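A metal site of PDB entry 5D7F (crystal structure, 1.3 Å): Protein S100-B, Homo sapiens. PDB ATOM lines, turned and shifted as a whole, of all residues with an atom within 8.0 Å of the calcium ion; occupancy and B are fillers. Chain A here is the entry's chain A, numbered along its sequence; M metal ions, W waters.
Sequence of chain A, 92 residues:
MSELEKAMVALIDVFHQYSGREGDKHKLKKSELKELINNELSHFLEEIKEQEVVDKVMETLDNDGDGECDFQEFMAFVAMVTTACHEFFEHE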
ATOM      1  N   PHE A  15      26.145  -4.080   3.771  1.00  0.00           N
ATOM      2  CA  PHE A  15      25.352  -4.283   4.970  1.00  0.00           C
ATOM      3  C   PHE A  15      25.691  -3.245   6.017  1.00  0.00           C
ATOM      4  O   PHE A  15      24.799  -2.613   6.618  1.00  0.00           O
ATOM      5  CB  PHE A  15      25.570  -5.698   5.550  1.00  0.00           C
ATOM      6  CG  PHE A  15      24.829  -5.903   6.864  1.00  0.00           C
ATOM      7  CD1 PHE A  15      23.467  -6.215   6.853  1.00  0.00           C
ATOM      8  CD2 PHE A  15      25.472  -5.741   8.093  1.00  0.00           C
ATOM      9  CE1 PHE A  15      22.756  -6.420   8.057  1.00  0.00           C
ATOM     10  CE2 PHE A  15      24.770  -5.901   9.302  1.00  0.00           C
ATOM     11  CZ  PHE A  15      23.439  -6.264   9.284  1.00  0.00           C
ATOM     12  N   HIS A  16      26.971  -3.026   6.231  1.00  0.00           N
ATOM     13  CA  HIS A  16      27.368  -2.131   7.306  1.00  0.00           C
ATOM     14  C   HIS A  16      27.155  -0.678   6.992  1.00  0.00           C
ATOM     15  O   HIS A  16      26.880   0.114   7.911  1.00  0.00           O
ATOM     16  CB  HIS A  16      28.791  -2.421   7.704  1.00  0.00           C
ATOM     17  CG  HIS A  16      28.897  -3.662   8.526  1.00  0.00           C
ATOM     18  ND1 HIS A  16      28.640  -3.674   9.876  1.00  0.00           N
ATOM     19  CD2 HIS A  16      29.171  -4.943   8.169  1.00  0.00           C
ATOM     20  CE1 HIS A  16      28.791  -4.900  10.330  1.00  0.00           C
ATOM     21  NE2 HIS A  16      29.118  -5.693   9.322  1.00  0.00           N
ATOM     22  N   GLN A  17      27.260  -0.336   5.713  1.00  0.00           N
ATOM     23  CA  GLN A  17      26.884   1.012   5.256  1.00  0.00           C
ATOM     24  C   GLN A  17      25.461   1.347   5.724  1.00  0.00           C
ATOM     25  O   GLN A  17      25.196   2.420   6.254  1.00  0.00           O
ATOM     26  CB  GLN A  17      26.976   1.097   3.723  1.00  0.00           C
ATOM     27  CG  GLN A  17      28.378   1.271   3.137  1.00  0.00           C
ATOM     28  CD  GLN A  17      28.466   0.902   1.634  1.00  0.00           C
ATOM     29  OE1 GLN A  17      27.435   0.800   0.936  1.00  0.00           O
ATOM     30  NE2 GLN A  17      29.683   0.669   1.144  1.00  0.00           N
ATOM     31  N   TYR A  18      24.523   0.426   5.546  1.00  0.00           N
ATOM     32  CA  TYR A  18      23.149   0.680   5.926  1.00  0.00           C
ATOM     33  C   TYR A  18      22.863   0.399   7.369  1.00  0.00           C
ATOM     34  O   TYR A  18      22.121   1.156   8.000  1.00  0.00           O
ATOM     35  CB  TYR A  18      22.215  -0.090   4.984  1.00  0.00           C
ATOM     36  CG  TYR A  18      22.133   0.568   3.627  1.00  0.00           C
ATOM     37  CD1 TYR A  18      23.096   0.305   2.629  1.00  0.00           C
ATOM     38  CD2 TYR A  18      21.133   1.510   3.368  1.00  0.00           C
ATOM     39  CE1 TYR A  18      23.066   0.967   1.411  1.00  0.00           C
ATOM     40  CE2 TYR A  18      21.103   2.172   2.150  1.00  0.00           C
ATOM     41  CZ  TYR A  18      22.054   1.918   1.184  1.00  0.00           C
ATOM     42  OH  TYR A  18      21.970   2.618   0.005  1.00  0.00           O
ATOM     43  N   SER A  19      23.440  -0.653   7.956  1.00  0.00           N
ATOM     44  CA  SER A  19      23.105  -0.998   9.339  1.00  0.00           C
ATOM     45  C   SER A  19      23.617   0.038  10.325  1.00  0.00           C
ATOM     46  O   SER A  19      23.022   0.211  11.390  1.00  0.00           O
ATOM     47  CB  SER A  19      23.667  -2.377   9.734  1.00  0.00           C
ATOM     48  OG  SER A  19      25.060  -2.383   9.708  1.00  0.00           O
ATOM     49  N   GLY A  20      24.715   0.696   9.960  1.00  0.00           N
ATOM     50  CA  GLY A  20      25.352   1.650  10.843  1.00  0.00           C
ATOM     51  C   GLY A  20      24.710   3.032  10.836  1.00  0.00           C
ATOM     52  O   GLY A  20      25.210   3.926  11.531  1.00  0.00           O
ATOM     53  N   ARG A  21      23.642   3.232  10.068  1.00  0.00           N
ATOM     54  CA  ARG A  21      23.025   4.571  10.007  1.00  0.00           C
ATOM     55  C   ARG A  21      22.368   4.987  11.346  1.00  0.00           C
ATOM     56  O   ARG A  21      22.533   6.137  11.795  1.00  0.00           O
ATOM     57  CB  ARG A  21      21.991   4.647   8.872  1.00  0.00           C
ATOM     58  CG  ARG A  21      22.639   4.569   7.509  1.00  0.00           C
ATOM     59  CD  ARG A  21      21.588   4.506   6.404  1.00  0.00           C
ATOM     60  NE  ARG A  21      22.198   4.656   5.100  1.00  0.00           N
ATOM     61  CZ  ARG A  21      21.517   4.999   4.021  1.00  0.00           C
ATOM     62  NH1 ARG A  21      20.202   5.208   4.105  1.00  0.00           N
ATOM     63  NH2 ARG A  21      22.127   5.162   2.865  1.00  0.00           N
ATOM     64  N   GLU A  22      21.604   4.075  11.956  1.00  0.00           N
ATOM     65  CA  GLU A  22      20.744   4.382  13.095  1.00  0.00           C
ATOM     66  C   GLU A  22      20.663   3.186  14.026  1.00  0.00           C
ATOM     67  O   GLU A  22      20.817   2.001  13.585  1.00  0.00           O
ATOM     68  CB  GLU A  22      19.335   4.744  12.613  1.00  0.00           C
ATOM     69  CG  GLU A  22      19.260   6.058  11.809  1.00  0.00           C
ATOM     70  CD  GLU A  22      17.858   6.396  11.292  1.00  0.00           C
ATOM     71  OE1 GLU A  22      16.866   5.954  11.907  1.00  0.00           O
ATOM     72  OE2 GLU A  22      17.745   7.110  10.271  1.00  0.00           O
ATOM     73  N   GLY A  23      20.467   3.488  15.308  1.00  0.00           N
ATOM     74  CA  GLY A  23      20.159   2.498  16.301  1.00  0.00           C
ATOM     75  C   GLY A  23      21.298   1.535  16.415  1.00  0.00           C
ATOM     76  O   GLY A  23      22.460   1.922  16.331  1.00  0.00           O
ATOM     77  N   ASP A  24      20.947   0.272  16.581  1.00  0.00           N
ATOM     78  CA  ASP A  24      21.917  -0.796  16.583  1.00  0.00           C
ATOM     79  C   ASP A  24      22.745  -0.736  15.290  1.00  0.00           C
ATOM     80  O   ASP A  24      22.204  -0.840  14.198  1.00  0.00           O
ATOM     81  CB  ASP A  24      21.165  -2.121  16.665  1.00  0.00           C
ATOM     82  CG  ASP A  24      22.083  -3.322  16.962  1.00  0.00           C
ATOM     83  OD1 ASP A  24      23.201  -3.398  16.419  1.00  0.00           O
ATOM     84  OD2 ASP A  24      21.689  -4.210  17.756  1.00  0.00           O
ATOM     85  N   LYS A  25      24.051  -0.602  15.409  1.00  0.00           N
ATOM     86  CA  LYS A  25      24.917  -0.478  14.234  1.00  0.00           C
ATOM     87  C   LYS A  25      25.150  -1.784  13.506  1.00  0.00           C
ATOM     88  O   LYS A  25      25.738  -1.800  12.422  1.00  0.00           O
ATOM     89  CB  LYS A  25      26.241   0.182  14.596  1.00  0.00           C
ATOM     90  CG  LYS A  25      26.042   1.626  15.052  1.00  0.00           C
ATOM     91  CD  LYS A  25      27.326   2.414  15.148  1.00  0.00           C
ATOM     92  CE  LYS A  25      27.045   3.864  15.533  1.00  0.00           C
ATOM     93  NZ  LYS A  25      26.262   4.566  14.466  1.00  0.00           N
ATOM     94  N   HIS A  26      24.713  -2.890  14.106  1.00  0.00           N
ATOM     95  CA  HIS A  26      24.947  -4.208  13.522  1.00  0.00           C
ATOM     96  C   HIS A  26      23.689  -4.805  12.927  1.00  0.00           C
ATOM     97  O   HIS A  26      23.696  -5.940  12.500  1.00  0.00           O
ATOM     98  CB  HIS A  26      25.515  -5.156  14.580  1.00  0.00           C
ATOM     99  CG  HIS A  26      26.875  -4.766  15.078  1.00  0.00           C
ATOM    100  ND1 HIS A  26      27.369  -3.482  14.967  1.00  0.00           N
ATOM    101  CD2 HIS A  26      27.842  -5.483  15.672  1.00  0.00           C
ATOM    102  CE1 HIS A  26      28.575  -3.429  15.491  1.00  0.00           C
ATOM    103  NE2 HIS A  26      28.887  -4.639  15.924  1.00  0.00           N
ATOM    104  N   LYS A  27      22.593  -4.035  12.931  1.00  0.00           N
ATOM    105  CA  LYS A  27      21.353  -4.527  12.391  1.00  0.00           C
ATOM    106  C   LYS A  27      20.675  -3.438  11.559  1.00  0.00           C
ATOM    107  O   LYS A  27      20.889  -2.201  11.819  1.00  0.00           O
ATOM    108  CB  LYS A  27      20.407  -4.936  13.510  1.00  0.00           C
ATOM    109  CG  LYS A  27      20.953  -6.045  14.419  1.00  0.00           C
ATOM    110  CD  LYS A  27      19.941  -6.393  15.503  1.00  0.00           C
ATOM    111  CE  LYS A  27      20.462  -7.456  16.504  1.00  0.00           C
ATOM    112  NZ  LYS A  27      19.428  -7.705  17.599  1.00  0.00           N
ATOM    113  N   LEU A  28      19.879  -3.912  10.603  1.00  0.00           N
ATOM    114  CA  LEU A  28      18.999  -3.089   9.772  1.00  0.00           C
ATOM    115  C   LEU A  28      17.631  -2.962  10.405  1.00  0.00           C
ATOM    116  O   LEU A  28      16.899  -3.943  10.530  1.00  0.00           O
ATOM    117  CB  LEU A  28      18.850  -3.713   8.368  1.00  0.00           C
ATOM    118  CG  LEU A  28      20.123  -3.926   7.576  1.00  0.00           C
ATOM    119  CD1 LEU A  28      19.851  -4.903   6.398  1.00  0.00           C
ATOM    120  CD2 LEU A  28      20.662  -2.619   7.018  1.00  0.00           C
ATOM    121  N   LYS A  29      17.250  -1.736  10.742  1.00  0.00           N
ATOM    122  CA  LYS A  29      15.834  -1.448  11.066  1.00  0.00           C
ATOM    123  C   LYS A  29      15.055  -1.264   9.751  1.00  0.00           C
ATOM    124  O   LYS A  29      15.647  -1.227   8.673  1.00  0.00           O
ATOM    125  CB  LYS A  29      15.730  -0.186  11.956  1.00  0.00           C
ATOM    126  CG  LYS A  29      16.224   1.061  11.296  1.00  0.00           C
ATOM    127  CD  LYS A  29      16.442   2.220  12.265  1.00  0.00           C
ATOM    128  CE  LYS A  29      15.135   2.689  12.772  1.00  0.00           C
ATOM    129  NZ  LYS A  29      14.563   3.729  11.853  1.00  0.00           N
ATOM    130  N   LYS A  30      13.733  -1.151   9.832  1.00  0.00           N
ATOM    131  CA  LYS A  30      12.947  -1.065   8.616  1.00  0.00           C
ATOM    132  C   LYS A  30      13.403  -0.003   7.647  1.00  0.00           C
ATOM    133  O   LYS A  30      13.498  -0.251   6.445  1.00  0.00           O
ATOM    134  CB  LYS A  30      11.459  -0.840   8.911  1.00  0.00           C
ATOM    135  CG  LYS A  30      10.737  -2.049   9.482  1.00  0.00           C
ATOM    136  CD  LYS A  30       9.311  -1.661   9.845  1.00  0.00           C
ATOM    137  CE  LYS A  30       8.478  -2.843  10.425  1.00  0.00           C
ATOM    138  NZ  LYS A  30       7.197  -2.317  10.946  1.00  0.00           N
ATOM    139  N   SER A  31      13.705   1.209   8.118  1.00  0.00           N
ATOM    140  CA  SER A  31      14.051   2.268   7.178  1.00  0.00           C
ATOM    141  C   SER A  31      15.387   1.953   6.513  1.00  0.00           C
ATOM    142  O   SER A  31      15.540   2.253   5.340  1.00  0.00           O
ATOM    143  CB  SER A  31      14.128   3.614   7.898  1.00  0.00           C
ATOM    144  OG  SER A  31      15.023   3.543   8.992  1.00  0.00           O
ATOM    145  N   GLU A  32      16.364   1.426   7.257  1.00  0.00           N
ATOM    146  CA  GLU A  32      17.667   1.076   6.678  1.00  0.00           C
ATOM    147  C   GLU A  32      17.504  -0.027   5.613  1.00  0.00           C
ATOM    148  O   GLU A  32      18.123   0.057   4.540  1.00  0.00           O
ATOM    149  CB  GLU A  32      18.641   0.621   7.784  1.00  0.00           C
ATOM    150  CG  GLU A  32      19.063   1.752   8.729  1.00  0.00           C
ATOM    151  CD  GLU A  32      19.730   1.192  10.001  1.00  0.00           C
ATOM    152  OE1 GLU A  32      19.521   0.011  10.383  1.00  0.00           O
ATOM    153  OE2 GLU A  32      20.543   1.931  10.594  1.00  0.00           O
ATOM    154  N   LEU A  33      16.698  -1.035   5.915  1.00  0.00           N
ATOM    155  CA  LEU A  33      16.442  -2.110   4.960  1.00  0.00           C
ATOM    156  C   LEU A  33      15.736  -1.598   3.705  1.00  0.00           C
ATOM    157  O   LEU A  33      16.097  -1.977   2.569  1.00  0.00           O
ATOM    158  CB  LEU A  33      15.598  -3.176   5.663  1.00  0.00           C
ATOM    159  CG  LEU A  33      15.162  -4.369   4.812  1.00  0.00           C
ATOM    160  CD1 LEU A  33      16.337  -5.118   4.221  1.00  0.00           C
ATOM    161  CD2 LEU A  33      14.238  -5.292   5.618  1.00  0.00           C
ATOM    162  N   GLU A  68      14.386  -6.440  13.605  1.00  0.00           N
ATOM    163  CA  GLU A  68      15.473  -5.944  12.777  1.00  0.00           C
ATOM    164  C   GLU A  68      16.081  -7.091  11.982  1.00  0.00           C
ATOM    165  O   GLU A  68      15.879  -8.303  12.305  1.00  0.00           O
ATOM    166  CB  GLU A  68      16.579  -5.291  13.592  1.00  0.00           C
ATOM    167  CG  GLU A  68      16.034  -4.113  14.459  1.00  0.00           C
ATOM    168  CD  GLU A  68      17.038  -2.996  14.693  1.00  0.00           C
ATOM    169  OE1 GLU A  68      17.930  -2.797  13.857  1.00  0.00           O
ATOM    170  OE2 GLU A  68      16.959  -2.309  15.707  1.00  0.00           O
ATOM    171  N   CYS A  69      16.845  -6.733  10.947  1.00  0.00           N
ATOM    172  CA  CYS A  69      17.532  -7.713  10.107  1.00  0.00           C
ATOM    173  C   CYS A  69      19.023  -7.689  10.408  1.00  0.00           C
ATOM    174  O   CYS A  69      19.720  -6.708  10.130  1.00  0.00           O
ATOM    175  CB  CYS A  69      17.234  -7.406   8.634  1.00  0.00           C
ATOM    176  SG  CYS A  69      17.997  -8.558   7.487  1.00  0.00           S
HETATM  177 CA    CA M   1      20.909   0.072  12.366  1.00  0.00          CA
HETATM  178  O   HOH W   1      18.885  -0.412  13.537  1.00  0.00           O
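The calcium ion is bound by the backbone carbonyl oxygen (O) of Glu 22, the backbone carbonyl oxygen (O) of Ser 19, the backbone carbonyl oxygen (O) of Lys 27, water W1, the side-chain carboxylate (OE1) of Glu 32, the backbone carbonyl oxygen (O) of Asp 24 and the side-chain carboxylate (OE2) of Glu 32.
The calcium ion has seven donor atoms within binding distance.
The nearest printed residue that does not touch the calcium ion is Gly 23 (4.3 Å).
The backbone NH (N) of Arg 21 lies close to the side-chain carboxylate (OE2) of Glu 32 (3.4 Å).
OG of Ser 19 lies within hydrogen-bond range of O of Phe 15, at 3.1 Å.
The backbone NH (N) of His 26 lies within hydrogen-bond range of the side-chain carboxylate (OD1) of Asp 24 (2.8 Å).
OE1 of Glu 32 lies close to N of Lys 29 (2.9 Å).
NZ of Lys 29 is in salt-bridge range of OE1 of Glu 22, at 3.2 Å.
OG of Ser 19 lies within hydrogen-bond range of O of Lys 25, at 2.9 Å.
Water W1 lies within hydrogen-bond range of OE1 of Glu 68 (2.6 Å) and N of Lys 29 (3.5 Å).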
